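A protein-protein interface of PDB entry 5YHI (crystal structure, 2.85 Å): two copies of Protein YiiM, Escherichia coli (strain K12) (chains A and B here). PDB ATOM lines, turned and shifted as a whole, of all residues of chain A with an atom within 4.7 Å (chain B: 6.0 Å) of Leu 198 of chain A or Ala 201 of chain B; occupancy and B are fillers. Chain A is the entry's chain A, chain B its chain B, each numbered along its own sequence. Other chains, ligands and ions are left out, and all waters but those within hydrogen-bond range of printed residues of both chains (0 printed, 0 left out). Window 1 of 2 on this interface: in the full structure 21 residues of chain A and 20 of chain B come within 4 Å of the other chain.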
ATOM      1  N   TYR A 194     -16.297   8.968 -22.596  1.00  0.00           N
ATOM      2  CA  TYR A 194     -15.178   9.691 -23.196  1.00  0.00           C
ATOM      3  C   TYR A 194     -15.688  10.787 -24.155  1.00  0.00           C
ATOM      4  O   TYR A 194     -15.128  11.872 -24.239  1.00  0.00           O
ATOM      5  CB  TYR A 194     -14.209   8.727 -23.896  1.00  0.00           C
ATOM      6  CG  TYR A 194     -13.679   7.651 -22.994  1.00  0.00           C
ATOM      7  CD1 TYR A 194     -13.411   7.897 -21.664  1.00  0.00           C
ATOM      8  CD2 TYR A 194     -13.408   6.384 -23.476  1.00  0.00           C
ATOM      9  CE1 TYR A 194     -12.940   6.905 -20.827  1.00  0.00           C
ATOM     10  CE2 TYR A 194     -12.916   5.365 -22.632  1.00  0.00           C
ATOM     11  CZ  TYR A 194     -12.697   5.641 -21.314  1.00  0.00           C
ATOM     12  OH  TYR A 194     -12.228   4.659 -20.464  1.00  0.00           O
ATOM     13  N   HIS A 195     -16.762  10.487 -24.863  1.00  0.00           N
ATOM     14  CA  HIS A 195     -17.417  11.466 -25.694  1.00  0.00           C
ATOM     15  C   HIS A 195     -17.877  12.655 -24.881  1.00  0.00           C
ATOM     16  O   HIS A 195     -17.769  13.815 -25.290  1.00  0.00           O
ATOM     17  CB  HIS A 195     -18.637  10.846 -26.324  1.00  0.00           C
ATOM     18  CG  HIS A 195     -19.352  11.760 -27.262  1.00  0.00           C
ATOM     19  ND1 HIS A 195     -20.247  12.729 -26.852  1.00  0.00           N
ATOM     20  CD2 HIS A 195     -19.285  11.857 -28.609  1.00  0.00           C
ATOM     21  CE1 HIS A 195     -20.711  13.369 -27.909  1.00  0.00           C
ATOM     22  NE2 HIS A 195     -20.143  12.860 -28.985  1.00  0.00           N
ATOM     23  N   ARG A 196     -18.444  12.343 -23.729  1.00  0.00           N
ATOM     24  CA  ARG A 196     -18.850  13.357 -22.802  1.00  0.00           C
ATOM     25  C   ARG A 196     -17.676  14.211 -22.364  1.00  0.00           C
ATOM     26  O   ARG A 196     -17.768  15.435 -22.372  1.00  0.00           O
ATOM     27  CB  ARG A 196     -19.492  12.718 -21.601  1.00  0.00           C
ATOM     28  CG  ARG A 196     -19.954  13.718 -20.538  1.00  0.00           C
ATOM     29  CD  ARG A 196     -21.032  13.104 -19.657  1.00  0.00           C
ATOM     30  NE  ARG A 196     -21.556  14.090 -18.723  1.00  0.00           N
ATOM     31  CZ  ARG A 196     -21.323  14.091 -17.411  1.00  0.00           C
ATOM     32  NH1 ARG A 196     -20.587  13.130 -16.820  1.00  0.00           N
ATOM     33  NH2 ARG A 196     -21.853  15.058 -16.678  1.00  0.00           N
ATOM     34  N   LEU A 197     -16.571  13.584 -21.992  1.00  0.00           N
ATOM     35  CA  LEU A 197     -15.442  14.357 -21.512  1.00  0.00           C
ATOM     36  C   LEU A 197     -14.875  15.218 -22.638  1.00  0.00           C
ATOM     37  O   LEU A 197     -14.566  16.394 -22.435  1.00  0.00           O
ATOM     38  CB  LEU A 197     -14.390  13.454 -20.891  1.00  0.00           C
ATOM     39  CG  LEU A 197     -13.200  14.139 -20.198  1.00  0.00           C
ATOM     40  CD1 LEU A 197     -13.616  15.326 -19.325  1.00  0.00           C
ATOM     41  CD2 LEU A 197     -12.297  13.142 -19.405  1.00  0.00           C
ATOM     42  N   LEU A 198     -14.772  14.657 -23.839  1.00  0.00           N
ATOM     43  CA  LEU A 198     -14.300  15.423 -25.011  1.00  0.00           C
ATOM     44  C   LEU A 198     -15.156  16.660 -25.312  1.00  0.00           C
ATOM     45  O   LEU A 198     -14.663  17.638 -25.848  1.00  0.00           O
ATOM     46  CB  LEU A 198     -14.169  14.517 -26.248  1.00  0.00           C
ATOM     47  CG  LEU A 198     -12.974  13.545 -26.204  1.00  0.00           C
ATOM     48  CD1 LEU A 198     -13.088  12.499 -27.270  1.00  0.00           C
ATOM     49  CD2 LEU A 198     -11.636  14.270 -26.327  1.00  0.00           C
ATOM     50  N   SER A 199     -16.429  16.628 -24.942  1.00  0.00           N
ATOM     51  CA  SER A 199     -17.330  17.797 -25.069  1.00  0.00           C
ATOM     52  C   SER A 199     -17.170  18.902 -24.051  1.00  0.00           C
ATOM     53  O   SER A 199     -17.823  19.912 -24.186  1.00  0.00           O
ATOM     54  CB  SER A 199     -18.764  17.335 -24.957  1.00  0.00           C
ATOM     55  OG  SER A 199     -18.934  16.214 -25.793  1.00  0.00           O
ATOM     56  N   ALA A 200     -16.321  18.721 -23.041  1.00  0.00           N
ATOM     57  CA  ALA A 200     -16.149  19.725 -21.996  1.00  0.00           C
ATOM     58  C   ALA A 200     -15.276  20.889 -22.463  1.00  0.00           C
ATOM     59  O   ALA A 200     -14.102  20.706 -22.747  1.00  0.00           O
ATOM     60  CB  ALA A 200     -15.546  19.098 -20.784  1.00  0.00           C
ATOM     61  N   ALA A 201     -15.856  22.079 -22.528  1.00  0.00           N
ATOM     62  CA  ALA A 201     -15.150  23.317 -22.822  1.00  0.00           C
ATOM     63  C   ALA A 201     -13.924  23.437 -21.955  1.00  0.00           C
ATOM     64  O   ALA A 201     -13.937  23.025 -20.804  1.00  0.00           O
ATOM     65  CB  ALA A 201     -16.063  24.505 -22.560  1.00  0.00           C
ATOM     66  N   LEU A 203     -11.152  21.771 -22.033  1.00  0.00           N
ATOM     67  CA  LEU A 203     -10.358  20.555 -21.800  1.00  0.00           C
ATOM     68  C   LEU A 203      -8.917  20.732 -22.314  1.00  0.00           C
ATOM     69  O   LEU A 203      -8.703  21.149 -23.427  1.00  0.00           O
ATOM     70  CB  LEU A 203     -11.014  19.317 -22.441  1.00  0.00           C
ATOM     71  CG  LEU A 203     -10.404  17.954 -22.070  1.00  0.00           C
ATOM     72  CD1 LEU A 203     -10.748  17.545 -20.633  1.00  0.00           C
ATOM     73  CD2 LEU A 203     -10.844  16.870 -23.031  1.00  0.00           C
ATOM     74  N   THR A 208      -7.500  15.817 -24.092  1.00  0.00           N
ATOM     75  CA  THR A 208      -8.212  15.590 -25.343  1.00  0.00           C
ATOM     76  C   THR A 208      -7.504  14.482 -26.104  1.00  0.00           C
ATOM     77  O   THR A 208      -8.136  13.544 -26.606  1.00  0.00           O
ATOM     78  CB  THR A 208      -8.288  16.869 -26.194  1.00  0.00           C
ATOM     79  OG1 THR A 208      -8.985  17.892 -25.459  1.00  0.00           O
ATOM     80  CG2 THR A 208      -8.989  16.602 -27.508  1.00  0.00           C
ATOM     81  N   MET A 211      -7.977  10.990 -24.296  1.00  0.00           N
ATOM     82  CA  MET A 211      -9.334  10.423 -24.380  1.00  0.00           C
ATOM     83  C   MET A 211      -9.676  10.040 -25.803  1.00  0.00           C
ATOM     84  O   MET A 211     -10.315   9.009 -26.027  1.00  0.00           O
ATOM     85  CB  MET A 211     -10.390  11.408 -23.854  1.00  0.00           C
ATOM     86  CG  MET A 211     -10.258  11.747 -22.399  1.00  0.00           C
ATOM     87  SD  MET A 211     -10.571  10.313 -21.397  1.00  0.00           S
ATOM     88  CE  MET A 211      -9.453  10.627 -20.013  1.00  0.00           C
ATOM     89  N   GLN A 212      -9.263  10.866 -26.758  1.00  0.00           N
ATOM     90  CA  GLN A 212      -9.522  10.536 -28.157  1.00  0.00           C
ATOM     91  C   GLN A 212      -8.831   9.209 -28.510  1.00  0.00           C
ATOM     92  O   GLN A 212      -9.379   8.398 -29.269  1.00  0.00           O
ATOM     93  CB  GLN A 212      -9.058  11.646 -29.102  1.00  0.00           C
ATOM     94  CG  GLN A 212      -9.272  11.323 -30.569  1.00  0.00           C
ATOM     95  CD  GLN A 212     -10.728  11.105 -30.937  1.00  0.00           C
ATOM     96  OE1 GLN A 212     -11.461  12.055 -31.288  1.00  0.00           O
ATOM     97  NE2 GLN A 212     -11.149   9.843 -30.912  1.00  0.00           N
ATOM     98  N   ARG A 215     -10.741   6.208 -27.416  1.00  0.00           N
ATOM     99  CA  ARG A 215     -11.877   5.957 -28.280  1.00  0.00           C
ATOM    100  C   ARG A 215     -11.487   5.237 -29.542  1.00  0.00           C
ATOM    101  O   ARG A 215     -12.225   4.379 -29.982  1.00  0.00           O
ATOM    102  CB  ARG A 215     -12.568   7.250 -28.658  1.00  0.00           C
ATOM    103  CG  ARG A 215     -13.157   7.991 -27.497  1.00  0.00           C
ATOM    104  CD  ARG A 215     -14.134   9.016 -27.951  1.00  0.00           C
ATOM    105  NE  ARG A 215     -15.383   8.404 -28.386  1.00  0.00           N
ATOM    106  CZ  ARG A 215     -16.314   9.007 -29.119  1.00  0.00           C
ATOM    107  NH1 ARG A 215     -16.151  10.253 -29.541  1.00  0.00           N
ATOM    108  NH2 ARG A 215     -17.418   8.360 -29.446  1.00  0.00           N
ATOM    109  N   MET B 106     -17.927  23.002 -34.228  1.00  0.00           N
ATOM    110  CA  MET B 106     -16.919  23.359 -33.244  1.00  0.00           C
ATOM    111  C   MET B 106     -16.491  22.130 -32.419  1.00  0.00           C
ATOM    112  O   MET B 106     -17.307  21.283 -32.055  1.00  0.00           O
ATOM    113  CB  MET B 106     -17.435  24.422 -32.296  1.00  0.00           C
ATOM    114  CG  MET B 106     -17.873  25.698 -32.947  1.00  0.00           C
ATOM    115  SD  MET B 106     -16.546  26.625 -33.672  1.00  0.00           S
ATOM    116  CE  MET B 106     -15.798  27.393 -32.225  1.00  0.00           C
ATOM    117  N   GLY B 107     -15.189  22.023 -32.171  1.00  0.00           N
ATOM    118  CA  GLY B 107     -14.657  20.889 -31.425  1.00  0.00           C
ATOM    119  C   GLY B 107     -14.549  19.582 -32.195  1.00  0.00           C
ATOM    120  O   GLY B 107     -14.130  18.571 -31.619  1.00  0.00           O
ATOM    121  N   ASP B 108     -14.911  19.575 -33.480  1.00  0.00           N
ATOM    122  CA  ASP B 108     -14.872  18.324 -34.232  1.00  0.00           C
ATOM    123  C   ASP B 108     -13.447  17.839 -34.200  1.00  0.00           C
ATOM    124  O   ASP B 108     -12.527  18.649 -34.339  1.00  0.00           O
ATOM    125  CB  ASP B 108     -15.307  18.516 -35.689  1.00  0.00           C
ATOM    126  CG  ASP B 108     -16.809  18.377 -35.902  1.00  0.00           C
ATOM    127  OD1 ASP B 108     -17.522  17.925 -34.988  1.00  0.00           O
ATOM    128  OD2 ASP B 108     -17.280  18.717 -37.015  1.00  0.00           O
ATOM    129  N   ILE B 109     -13.249  16.541 -33.990  1.00  0.00           N
ATOM    130  CA  ILE B 109     -11.916  15.971 -34.111  1.00  0.00           C
ATOM    131  C   ILE B 109     -11.838  15.073 -35.336  1.00  0.00           C
ATOM    132  O   ILE B 109     -12.673  14.185 -35.504  1.00  0.00           O
ATOM    133  CB  ILE B 109     -11.505  15.177 -32.862  1.00  0.00           C
ATOM    134  CG1 ILE B 109     -11.529  16.069 -31.611  1.00  0.00           C
ATOM    135  CG2 ILE B 109     -10.124  14.564 -33.068  1.00  0.00           C
ATOM    136  CD1 ILE B 109     -11.339  15.298 -30.357  1.00  0.00           C
ATOM    137  N   GLN B 118      -8.380  19.306 -34.242  1.00  0.00           N
ATOM    138  CA  GLN B 118      -9.660  19.734 -33.675  1.00  0.00           C
ATOM    139  C   GLN B 118     -10.017  21.155 -34.151  1.00  0.00           C
ATOM    140  O   GLN B 118      -9.153  22.037 -34.177  1.00  0.00           O
ATOM    141  CB  GLN B 118      -9.613  19.708 -32.147  1.00  0.00           C
ATOM    142  CG  GLN B 118     -10.987  19.861 -31.509  1.00  0.00           C
ATOM    143  CD  GLN B 118     -10.925  19.933 -30.021  1.00  0.00           C
ATOM    144  OE1 GLN B 118     -10.078  20.631 -29.460  1.00  0.00           O
ATOM    145  NE2 GLN B 118     -11.831  19.217 -29.355  1.00  0.00           N
ATOM    146  N   VAL B 119     -11.287  21.354 -34.506  1.00  0.00           N
ATOM    147  CA  VAL B 119     -11.756  22.617 -35.034  1.00  0.00           C
ATOM    148  C   VAL B 119     -11.838  23.582 -33.874  1.00  0.00           C
ATOM    149  O   VAL B 119     -12.550  23.296 -32.900  1.00  0.00           O
ATOM    150  CB  VAL B 119     -13.164  22.483 -35.645  1.00  0.00           C
ATOM    151  CG1 VAL B 119     -13.738  23.861 -35.927  1.00  0.00           C
ATOM    152  CG2 VAL B 119     -13.134  21.612 -36.900  1.00  0.00           C
ATOM    153  N   SER B 170     -14.621  12.292 -33.928  1.00  0.00           N
ATOM    154  CA  SER B 170     -15.474  12.742 -32.833  1.00  0.00           C
ATOM    155  C   SER B 170     -16.167  14.033 -33.149  1.00  0.00           C
ATOM    156  O   SER B 170     -15.494  14.997 -33.504  1.00  0.00           O
ATOM    157  CB  SER B 170     -14.669  12.968 -31.563  1.00  0.00           C
ATOM    158  OG  SER B 170     -14.339  11.737 -30.960  1.00  0.00           O
ATOM    159  N   VAL B 172     -18.453  16.535 -30.953  1.00  0.00           N
ATOM    160  CA  VAL B 172     -18.713  16.743 -29.508  1.00  0.00           C
ATOM    161  C   VAL B 172     -19.472  18.049 -29.183  1.00  0.00           C
ATOM    162  O   VAL B 172     -19.411  18.570 -28.064  1.00  0.00           O
ATOM    163  CB  VAL B 172     -17.379  16.710 -28.720  1.00  0.00           C
ATOM    164  CG1 VAL B 172     -16.782  15.330 -28.786  1.00  0.00           C
ATOM    165  CG2 VAL B 172     -16.399  17.776 -29.243  1.00  0.00           C
ATOM    166  N   SER B 173     -20.222  18.554 -30.153  1.00  0.00           N
ATOM    167  CA  SER B 173     -20.848  19.859 -30.043  1.00  0.00           C
ATOM    168  C   SER B 173     -21.989  20.038 -31.031  1.00  0.00           C
ATOM    169  O   SER B 173     -22.126  19.320 -32.029  1.00  0.00           O
ATOM    170  CB  SER B 173     -19.801  20.934 -30.288  1.00  0.00           C
ATOM    171  OG  SER B 173     -20.355  22.147 -30.726  1.00  0.00           O
ATOM    172  N   LEU B 197     -21.648  29.596 -26.948  1.00  0.00           N
ATOM    173  CA  LEU B 197     -20.386  29.473 -27.659  1.00  0.00           C
ATOM    174  C   LEU B 197     -19.259  29.078 -26.718  1.00  0.00           C
ATOM    175  O   LEU B 197     -18.464  28.184 -27.032  1.00  0.00           O
ATOM    176  CB  LEU B 197     -20.037  30.768 -28.420  1.00  0.00           C
ATOM    177  CG  LEU B 197     -18.791  30.759 -29.332  1.00  0.00           C
ATOM    178  CD1 LEU B 197     -18.664  29.432 -30.126  1.00  0.00           C
ATOM    179  CD2 LEU B 197     -18.742  32.011 -30.279  1.00  0.00           C
ATOM    180  N   LEU B 198     -19.207  29.717 -25.550  1.00  0.00           N
ATOM    181  CA  LEU B 198     -18.225  29.337 -24.504  1.00  0.00           C
ATOM    182  C   LEU B 198     -18.302  27.870 -24.079  1.00  0.00           C
ATOM    183  O   LEU B 198     -17.330  27.334 -23.615  1.00  0.00           O
ATOM    184  CB  LEU B 198     -18.358  30.245 -23.278  1.00  0.00           C
ATOM    185  CG  LEU B 198     -17.879  31.687 -23.492  1.00  0.00           C
ATOM    186  CD1 LEU B 198     -18.349  32.558 -22.343  1.00  0.00           C
ATOM    187  CD2 LEU B 198     -16.389  31.748 -23.622  1.00  0.00           C
ATOM    188  N   SER B 199     -19.459  27.238 -24.249  1.00  0.00           N
ATOM    189  CA  SER B 199     -19.635  25.805 -24.020  1.00  0.00           C
ATOM    190  C   SER B 199     -19.172  24.899 -25.148  1.00  0.00           C
ATOM    191  O   SER B 199     -19.342  23.710 -25.054  1.00  0.00           O
ATOM    192  CB  SER B 199     -21.117  25.486 -23.794  1.00  0.00           C
ATOM    193  OG  SER B 199     -21.695  26.290 -22.776  1.00  0.00           O
ATOM    194  N   ALA B 200     -18.635  25.426 -26.230  1.00  0.00           N
ATOM    195  CA  ALA B 200     -18.178  24.575 -27.333  1.00  0.00           C
ATOM    196  C   ALA B 200     -16.795  23.950 -27.087  1.00  0.00           C
ATOM    197  O   ALA B 200     -15.797  24.633 -26.869  1.00  0.00           O
ATOM    198  CB  ALA B 200     -18.168  25.368 -28.611  1.00  0.00           C
ATOM    199  N   ALA B 201     -16.743  22.627 -27.112  1.00  0.00           N
ATOM    200  CA  ALA B 201     -15.468  21.901 -27.045  1.00  0.00           C
ATOM    201  C   ALA B 201     -14.511  22.424 -28.083  1.00  0.00           C
ATOM    202  O   ALA B 201     -14.918  22.746 -29.187  1.00  0.00           O
ATOM    203  CB  ALA B 201     -15.674  20.403 -27.234  1.00  0.00           C
ATOM    204  N   GLY B 202     -13.248  22.539 -27.687  1.00  0.00           N
ATOM    205  CA  GLY B 202     -12.187  22.964 -28.559  1.00  0.00           C
ATOM    206  C   GLY B 202     -12.028  24.449 -28.810  1.00  0.00           C
ATOM    207  O   GLY B 202     -11.005  24.850 -29.362  1.00  0.00           O
ATOM    208  N   LEU B 203     -13.001  25.272 -28.414  1.00  0.00           N
ATOM    209  CA  LEU B 203     -12.956  26.714 -28.680  1.00  0.00           C
ATOM    210  C   LEU B 203     -11.571  27.272 -28.400  1.00  0.00           C
ATOM    211  O   LEU B 203     -10.986  27.008 -27.369  1.00  0.00           O
ATOM    212  CB  LEU B 203     -13.977  27.483 -27.840  1.00  0.00           C
ATOM    213  CG  LEU B 203     -14.205  28.955 -28.230  1.00  0.00           C
ATOM    214  CD1 LEU B 203     -14.907  29.158 -29.650  1.00  0.00           C
ATOM    215  CD2 LEU B 203     -14.969  29.684 -27.127  1.00  0.00           C
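The side-chain hydroxyl (OG) of Ser 199 of chain A is in hydrogen-bond range of the backbone carbonyl oxygen (O) of Val 172 of chain B, at 3.3 Å. OG of Ser 170 of chain B is in hydrogen-bond range of OE1 of Gln 212 of chain A (2.9 Å). The guanidinium group (NH1) of Arg 215 of chain A lies within hydrogen-bond range of the side-chain hydroxyl (OG) of Ser 170 of chain B.
The backbone NH (N) of Gly 107 of chain B lies close to the backbone carbonyl oxygen (O) of Ala 201 of chain B (3.1 Å). The backbone carbonyl oxygen (O) of His 195 of chain A lies within hydrogen-bond range of the side-chain hydroxyl (OG) of Ser 199 of chain A (2.7 Å). N of Ile 109 of chain B is in hydrogen-bond range of O of Ser 170 of chain B (2.8 Å).
O of His 195 of chain A touches CG1 of Val 172 of chain B, 3.9 Å away. Leu 198 of chain A touches Ser 170 of chain B (CD1 to OG, 3.97 Å). CB of Leu 198 of chain A touches CG1 of Val 172 of chain B (3.7 Å). O of Leu 198 of chain A touches CB of Ala 201 of chain B, at 3.3 Å. Ala 201 of chain B touches Ser 199 of chain A (CB to O, 3.8 Å). O of Leu 198 of chain B touches CB of Ala 201 of chain A, 3.3 Å away. CD1 of Ile 109 of chain B touches CG2 of Thr 208 of chain A, at 3.9 Å. Ile 109 of chain B touches Gln 212 of chain A.
Of chain B, only Ser 170, Val 172 and Ala 201 come within 4 Å of Leu 198 of chain A. Of chain A, only Leu 198 (3.3 Å) and Ser 199 (3.8 Å) come within 4 Å of Ala 201 of chain B. Of the printed residues of chain A, Leu 198 of chain B touches Ala 201 (3.3 Å). Of the printed residues of chain B, Ala 201 of chain A touches Leu 198. Of the printed residues of chain B, Ser 199 of chain A touches Val 172 (3.3 Å) and Ala 201 (3.8 Å). Printed residues of chain A within 4 Å of Val 172 of chain B: His 195, Leu 198 and Ser 199. The nearest residue of chain B that does not touch Leu 198 of chain A is Ile 109 of chain B (4.2 Å).
Of the 16 printed residues of chain B, 5 touch a printed residue of chain A. Printed residues of chain B that touch a printed residue of chain A: Ile 109, Ser 170, Val 172, Leu 198 and Ala 201. Printed residues of chain A that touch a printed residue of chain B: His 195, Leu 198, Ser 199, Ala 201, Thr 208, Gln 212 and Arg 215. Along chain A the printed residues that touch a printed residue of chain B span positions 195 to 215. Among the printed residues, no Asp or Glu carboxylate lies within 4 Å of a Lys or Arg side-chain nitrogen of the other chain.
Leu 198 of chain A touches Ala 201 of chain B, and with the chains exchanged Ala 201 of chain A touches Leu 198 of chain B. Ser 199 of chain A touches Ala 201 of chain B, but with the chains exchanged Ala 201 of chain A does not touch Ser 199 of chain B (4.1 Å). Of the 11 pairs that touch across the chains among the printed residues, 2 have their exchanged pair printed and touching as well.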
